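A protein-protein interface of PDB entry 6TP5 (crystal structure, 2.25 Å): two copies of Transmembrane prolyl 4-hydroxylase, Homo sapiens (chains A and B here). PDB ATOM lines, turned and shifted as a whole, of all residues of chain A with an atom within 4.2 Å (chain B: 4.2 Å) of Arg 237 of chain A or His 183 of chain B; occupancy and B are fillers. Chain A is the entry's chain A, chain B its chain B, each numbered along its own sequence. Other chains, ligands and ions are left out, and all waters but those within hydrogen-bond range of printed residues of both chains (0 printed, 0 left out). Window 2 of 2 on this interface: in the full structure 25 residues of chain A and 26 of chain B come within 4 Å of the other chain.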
ATOM      1  N   LEU A  87      -3.909  13.923  11.000  1.00  0.00           N
ATOM      2  CA  LEU A  87      -4.032  13.481  12.378  1.00  0.00           C
ATOM      3  C   LEU A  87      -5.430  12.930  12.639  1.00  0.00           C
ATOM      4  O   LEU A  87      -6.374  13.168  11.883  1.00  0.00           O
ATOM      5  CB  LEU A  87      -3.729  14.628  13.343  1.00  0.00           C
ATOM      6  CG  LEU A  87      -2.348  15.275  13.255  1.00  0.00           C
ATOM      7  CD1 LEU A  87      -2.272  16.449  14.192  1.00  0.00           C
ATOM      8  CD2 LEU A  87      -1.268  14.279  13.589  1.00  0.00           C
ATOM      9  N   SER A 194      -6.093  15.092  22.555  1.00  0.00           N
ATOM     10  CA  SER A 194      -5.067  15.442  21.577  1.00  0.00           C
ATOM     11  C   SER A 194      -5.391  14.731  20.268  1.00  0.00           C
ATOM     12  O   SER A 194      -6.341  13.946  20.184  1.00  0.00           O
ATOM     13  CB  SER A 194      -3.678  15.082  22.107  1.00  0.00           C
ATOM     14  OG  SER A 194      -3.466  13.684  22.012  1.00  0.00           O
ATOM     15  N   HIS A 195      -4.609  15.046  19.234  1.00  0.00           N
ATOM     16  CA  HIS A 195      -4.634  14.350  17.954  1.00  0.00           C
ATOM     17  C   HIS A 195      -3.243  13.802  17.674  1.00  0.00           C
ATOM     18  O   HIS A 195      -2.243  14.345  18.157  1.00  0.00           O
ATOM     19  CB  HIS A 195      -5.057  15.276  16.805  1.00  0.00           C
ATOM     20  CG  HIS A 195      -6.532  15.518  16.728  1.00  0.00           C
ATOM     21  ND1 HIS A 195      -7.230  16.186  17.710  1.00  0.00           N
ATOM     22  CD2 HIS A 195      -7.440  15.196  15.775  1.00  0.00           C
ATOM     23  CE1 HIS A 195      -8.505  16.255  17.373  1.00  0.00           C
ATOM     24  NE2 HIS A 195      -8.659  15.661  16.204  1.00  0.00           N
ATOM     25  N   VAL A 236       2.238  13.796  18.103  1.00  0.00           N
ATOM     26  CA  VAL A 236       1.056  14.248  18.829  1.00  0.00           C
ATOM     27  C   VAL A 236       0.940  15.760  18.710  1.00  0.00           C
ATOM     28  O   VAL A 236       1.925  16.487  18.902  1.00  0.00           O
ATOM     29  CB  VAL A 236       1.117  13.831  20.310  1.00  0.00           C
ATOM     30  CG1 VAL A 236      -0.075  14.396  21.074  1.00  0.00           C
ATOM     31  CG2 VAL A 236       1.185  12.312  20.437  1.00  0.00           C
ATOM     32  N   ARG A 237      -0.268  16.233  18.413  1.00  0.00           N
ATOM     33  CA  ARG A 237      -0.605  17.648  18.454  1.00  0.00           C
ATOM     34  C   ARG A 237      -1.580  17.896  19.596  1.00  0.00           C
ATOM     35  O   ARG A 237      -2.705  17.387  19.576  1.00  0.00           O
ATOM     36  CB  ARG A 237      -1.217  18.110  17.134  1.00  0.00           C
ATOM     37  CG  ARG A 237      -1.721  19.547  17.166  1.00  0.00           C
ATOM     38  CD  ARG A 237      -2.574  19.865  15.942  1.00  0.00           C
ATOM     39  NE  ARG A 237      -2.935  21.277  15.874  1.00  0.00           N
ATOM     40  CZ  ARG A 237      -3.923  21.839  16.572  1.00  0.00           C
ATOM     41  NH1 ARG A 237      -4.657  21.108  17.407  1.00  0.00           N
ATOM     42  NH2 ARG A 237      -4.181  23.137  16.432  1.00  0.00           N
ATOM     43  N   TYR A 238      -1.139  18.664  20.588  1.00  0.00           N
ATOM     44  CA  TYR A 238      -2.020  19.224  21.609  1.00  0.00           C
ATOM     45  C   TYR A 238      -2.435  20.616  21.151  1.00  0.00           C
ATOM     46  O   TYR A 238      -1.592  21.515  21.042  1.00  0.00           O
ATOM     47  CB  TYR A 238      -1.319  19.312  22.964  1.00  0.00           C
ATOM     48  CG  TYR A 238      -0.993  17.989  23.602  1.00  0.00           C
ATOM     49  CD1 TYR A 238      -1.931  17.321  24.374  1.00  0.00           C
ATOM     50  CD2 TYR A 238       0.266  17.413  23.451  1.00  0.00           C
ATOM     51  CE1 TYR A 238      -1.632  16.110  24.970  1.00  0.00           C
ATOM     52  CE2 TYR A 238       0.572  16.201  24.044  1.00  0.00           C
ATOM     53  CZ  TYR A 238      -0.382  15.555  24.800  1.00  0.00           C
ATOM     54  OH  TYR A 238      -0.094  14.356  25.399  1.00  0.00           O
ATOM     55  N   GLY A 239      -3.722  20.803  20.877  1.00  0.00           N
ATOM     56  CA  GLY A 239      -4.213  22.139  20.608  1.00  0.00           C
ATOM     57  C   GLY A 239      -4.358  22.940  21.886  1.00  0.00           C
ATOM     58  O   GLY A 239      -4.236  22.416  22.996  1.00  0.00           O
ATOM     59  N   THR A 369      -0.338  25.850  20.295  1.00  0.00           N
ATOM     60  CA  THR A 369      -0.356  24.404  20.166  1.00  0.00           C
ATOM     61  C   THR A 369       0.970  23.821  20.638  1.00  0.00           C
ATOM     62  O   THR A 369       2.006  24.491  20.629  1.00  0.00           O
ATOM     63  CB  THR A 369      -0.642  23.957  18.726  1.00  0.00           C
ATOM     64  OG1 THR A 369       0.487  24.246  17.906  1.00  0.00           O
ATOM     65  CG2 THR A 369      -1.877  24.667  18.172  1.00  0.00           C
ATOM     66  N   LYS A 370       0.913  22.568  21.075  1.00  0.00           N
ATOM     67  CA  LYS A 370       2.079  21.826  21.530  1.00  0.00           C
ATOM     68  C   LYS A 370       2.231  20.601  20.639  1.00  0.00           C
ATOM     69  O   LYS A 370       1.307  19.784  20.531  1.00  0.00           O
ATOM     70  CB  LYS A 370       1.943  21.426  23.000  1.00  0.00           C
ATOM     71  CG  LYS A 370       2.825  20.267  23.426  1.00  0.00           C
ATOM     72  CD  LYS A 370       2.663  19.987  24.918  1.00  0.00           C
ATOM     73  CE  LYS A 370       3.287  18.634  25.323  1.00  0.00           C
ATOM     74  NZ  LYS A 370       3.131  18.397  26.791  1.00  0.00           N
ATOM     75  N   TRP A 371       3.380  20.498  19.980  1.00  0.00           N
ATOM     76  CA  TRP A 371       3.713  19.379  19.115  1.00  0.00           C
ATOM     77  C   TRP A 371       4.807  18.561  19.777  1.00  0.00           C
ATOM     78  O   TRP A 371       5.836  19.114  20.181  1.00  0.00           O
ATOM     79  CB  TRP A 371       4.209  19.861  17.753  1.00  0.00           C
ATOM     80  CG  TRP A 371       3.167  20.429  16.859  1.00  0.00           C
ATOM     81  CD1 TRP A 371       2.791  21.737  16.764  1.00  0.00           C
ATOM     82  CD2 TRP A 371       2.383  19.715  15.901  1.00  0.00           C
ATOM     83  NE1 TRP A 371       1.812  21.880  15.813  1.00  0.00           N
ATOM     84  CE2 TRP A 371       1.542  20.656  15.265  1.00  0.00           C
ATOM     85  CE3 TRP A 371       2.303  18.374  15.521  1.00  0.00           C
ATOM     86  CZ2 TRP A 371       0.631  20.296  14.267  1.00  0.00           C
ATOM     87  CZ3 TRP A 371       1.400  18.017  14.525  1.00  0.00           C
ATOM     88  CH2 TRP A 371       0.578  18.977  13.912  1.00  0.00           C
ATOM     89  N   TRP B 139     -13.245  27.641  12.915  1.00  0.00           N
ATOM     90  CA  TRP B 139     -12.171  27.656  13.892  1.00  0.00           C
ATOM     91  C   TRP B 139     -12.018  29.060  14.464  1.00  0.00           C
ATOM     92  O   TRP B 139     -12.271  30.062  13.790  1.00  0.00           O
ATOM     93  CB  TRP B 139     -10.858  27.202  13.258  1.00  0.00           C
ATOM     94  CG  TRP B 139     -10.895  25.811  12.705  1.00  0.00           C
ATOM     95  CD1 TRP B 139     -10.836  25.450  11.391  1.00  0.00           C
ATOM     96  CD2 TRP B 139     -10.989  24.591  13.453  1.00  0.00           C
ATOM     97  NE1 TRP B 139     -10.891  24.081  11.273  1.00  0.00           N
ATOM     98  CE2 TRP B 139     -10.989  23.531  12.523  1.00  0.00           C
ATOM     99  CE3 TRP B 139     -11.077  24.293  14.819  1.00  0.00           C
ATOM    100  CZ2 TRP B 139     -11.073  22.196  12.915  1.00  0.00           C
ATOM    101  CZ3 TRP B 139     -11.165  22.967  15.205  1.00  0.00           C
ATOM    102  CH2 TRP B 139     -11.160  21.935  14.257  1.00  0.00           C
ATOM    103  N   TYR B 179      -4.293  23.980   3.841  1.00  0.00           N
ATOM    104  CA  TYR B 179      -4.026  23.970   5.275  1.00  0.00           C
ATOM    105  C   TYR B 179      -5.329  23.863   6.054  1.00  0.00           C
ATOM    106  O   TYR B 179      -5.435  23.078   7.005  1.00  0.00           O
ATOM    107  CB  TYR B 179      -3.253  25.221   5.681  1.00  0.00           C
ATOM    108  CG  TYR B 179      -2.845  25.234   7.141  1.00  0.00           C
ATOM    109  CD1 TYR B 179      -3.709  25.712   8.122  1.00  0.00           C
ATOM    110  CD2 TYR B 179      -1.605  24.752   7.542  1.00  0.00           C
ATOM    111  CE1 TYR B 179      -3.348  25.714   9.469  1.00  0.00           C
ATOM    112  CE2 TYR B 179      -1.234  24.746   8.886  1.00  0.00           C
ATOM    113  CZ  TYR B 179      -2.109  25.227   9.844  1.00  0.00           C
ATOM    114  OH  TYR B 179      -1.745  25.222  11.173  1.00  0.00           O
ATOM    115  N   MET B 180      -6.340  24.640   5.657  1.00  0.00           N
ATOM    116  CA  MET B 180      -7.655  24.509   6.269  1.00  0.00           C
ATOM    117  C   MET B 180      -8.291  23.168   5.918  1.00  0.00           C
ATOM    118  O   MET B 180      -9.008  22.589   6.737  1.00  0.00           O
ATOM    119  CB  MET B 180      -8.553  25.661   5.826  1.00  0.00           C
ATOM    120  CG  MET B 180      -7.896  27.022   5.940  1.00  0.00           C
ATOM    121  SD  MET B 180      -7.706  27.568   7.642  1.00  0.00           S
ATOM    122  CE  MET B 180      -9.408  27.499   8.191  1.00  0.00           C
ATOM    123  N   ARG B 181      -8.046  22.673   4.700  1.00  0.00           N
ATOM    124  CA  ARG B 181      -8.431  21.311   4.350  1.00  0.00           C
ATOM    125  C   ARG B 181      -7.973  20.338   5.431  1.00  0.00           C
ATOM    126  O   ARG B 181      -8.790  19.631   6.038  1.00  0.00           O
ATOM    127  CB  ARG B 181      -7.816  20.922   3.003  1.00  0.00           C
ATOM    128  CG  ARG B 181      -8.713  20.177   2.020  1.00  0.00           C
ATOM    129  CD  ARG B 181      -9.776  21.082   1.445  1.00  0.00           C
ATOM    130  NE  ARG B 181      -9.227  21.959   0.413  1.00  0.00           N
ATOM    131  CZ  ARG B 181      -9.942  22.864  -0.244  1.00  0.00           C
ATOM    132  NH1 ARG B 181      -9.374  23.634  -1.165  1.00  0.00           N
ATOM    133  NH2 ARG B 181     -11.234  22.998   0.024  1.00  0.00           N
ATOM    134  N   SER B 182      -6.658  20.326   5.710  1.00  0.00           N
ATOM    135  CA  SER B 182      -6.038  19.313   6.556  1.00  0.00           C
ATOM    136  C   SER B 182      -6.166  19.618   8.047  1.00  0.00           C
ATOM    137  O   SER B 182      -5.876  18.739   8.860  1.00  0.00           O
ATOM    138  CB  SER B 182      -4.527  19.207   6.195  1.00  0.00           C
ATOM    139  OG  SER B 182      -3.839  20.378   6.594  1.00  0.00           O
ATOM    140  N   HIS B 183      -6.605  20.815   8.417  1.00  0.00           N
ATOM    141  CA  HIS B 183      -6.604  21.222   9.816  1.00  0.00           C
ATOM    142  C   HIS B 183      -7.593  20.392  10.631  1.00  0.00           C
ATOM    143  O   HIS B 183      -8.804  20.428  10.386  1.00  0.00           O
ATOM    144  CB  HIS B 183      -6.941  22.702   9.933  1.00  0.00           C
ATOM    145  CG  HIS B 183      -6.593  23.299  11.259  1.00  0.00           C
ATOM    146  ND1 HIS B 183      -5.305  23.323  11.748  1.00  0.00           N
ATOM    147  CD2 HIS B 183      -7.365  23.896  12.197  1.00  0.00           C
ATOM    148  CE1 HIS B 183      -5.301  23.907  12.934  1.00  0.00           C
ATOM    149  NE2 HIS B 183      -6.538  24.265  13.228  1.00  0.00           N
ATOM    150  N   LYS B 184      -7.071  19.638  11.593  1.00  0.00           N
ATOM    151  CA  LYS B 184      -7.870  18.927  12.578  1.00  0.00           C
ATOM    152  C   LYS B 184      -7.487  19.456  13.953  1.00  0.00           C
ATOM    153  O   LYS B 184      -6.304  19.468  14.308  1.00  0.00           O
ATOM    154  CB  LYS B 184      -7.642  17.411  12.491  1.00  0.00           C
ATOM    155  CG  LYS B 184      -8.362  16.708  11.336  1.00  0.00           C
ATOM    156  CD  LYS B 184      -9.827  16.419  11.679  1.00  0.00           C
ATOM    157  CE  LYS B 184      -9.961  15.462  12.864  1.00  0.00           C
ATOM    158  NZ  LYS B 184     -11.259  15.609  13.598  1.00  0.00           N
ATOM    159  N   ALA B 185      -8.481  19.908  14.717  1.00  0.00           N
ATOM    160  CA  ALA B 185      -8.223  20.555  15.992  1.00  0.00           C
ATOM    161  C   ALA B 185      -9.383  20.280  16.943  1.00  0.00           C
ATOM    162  O   ALA B 185     -10.452  19.818  16.537  1.00  0.00           O
ATOM    163  CB  ALA B 185      -8.000  22.060  15.809  1.00  0.00           C
ATOM    164  N   GLU B 189     -10.802  24.802  20.245  1.00  0.00           N
ATOM    165  CA  GLU B 189     -10.284  25.736  19.252  1.00  0.00           C
ATOM    166  C   GLU B 189     -11.373  26.243  18.322  1.00  0.00           C
ATOM    167  O   GLU B 189     -11.072  26.934  17.348  1.00  0.00           O
ATOM    168  CB  GLU B 189      -9.156  25.082  18.451  1.00  0.00           C
ATOM    169  CG  GLU B 189      -8.205  24.296  19.343  1.00  0.00           C
ATOM    170  CD  GLU B 189      -6.942  23.827  18.646  1.00  0.00           C
ATOM    171  OE1 GLU B 189      -6.173  24.675  18.146  1.00  0.00           O
ATOM    172  OE2 GLU B 189      -6.711  22.598  18.615  1.00  0.00           O
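No position is printed for both chains.
Of the printed residues of chain B, His 195 of chain A touches Lys 184 (3.6 Å).
Of chain B, only His 183 (3.8 Å), Lys 184 (3.9 Å), Ala 185 (3.8 Å) and Glu 189 (2.8 Å) come within 4 Å of Arg 237 of chain A.
Of the printed residues of chain B, Gly 239 of chain A touches Glu 189 (3.2 Å).
Of chain A, only Arg 237 (3.8 Å) comes within 4 Å of His 183 of chain B.
Printed residues of chain A within 4 Å of Lys 184 of chain B: His 195 (3.6 Å) and Arg 237 (3.9 Å).
Of the printed residues of chain A, Ala 185 of chain B touches Arg 237.
Printed residues of chain A within 4 Å of Glu 189 of chain B: Arg 237 and Gly 239.
The nearest printed residue of chain B that does not touch Arg 237 of chain A is Tyr 179 of chain B (6.2 Å).
Of the 9 printed residues of chain B, 4 touch a printed residue of chain A.
Printed residues of chain B that touch a printed residue of chain A: His 183, Lys 184, Ala 185 and Glu 189.
Hydrophobic or aromatic side chains of chain B within 4 Å of the printed part of chain A: His 183 and Ala 185.
Among the printed residues, Asp or Glu carboxylates within 4 Å of a Lys or Arg side-chain nitrogen of the other chain: Arg 237 of chain A with Glu 189 of chain B (2.8 Å).
Among the printed residues, pairs that only touch across the chains: Gly 239 of chain A with Glu 189 of chain B (3.2 Å), His 195 of chain A with Lys 184 of chain B (3.6 Å), Arg 237 of chain A with His 183 of chain B (3.8 Å), Arg 237 of chain A with Ala 185 of chain B (3.8 Å) and Arg 237 of chain A with Lys 184 of chain B (3.9 Å).
O of His 195 of chain A is in hydrogen-bond range of N of Arg 237 of chain A (2.7 Å).
The side-chain carboxylate of Glu 189 of chain B lies within salt-bridge range of the guanidinium group of Arg 237 of chain A (2.8 Å).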
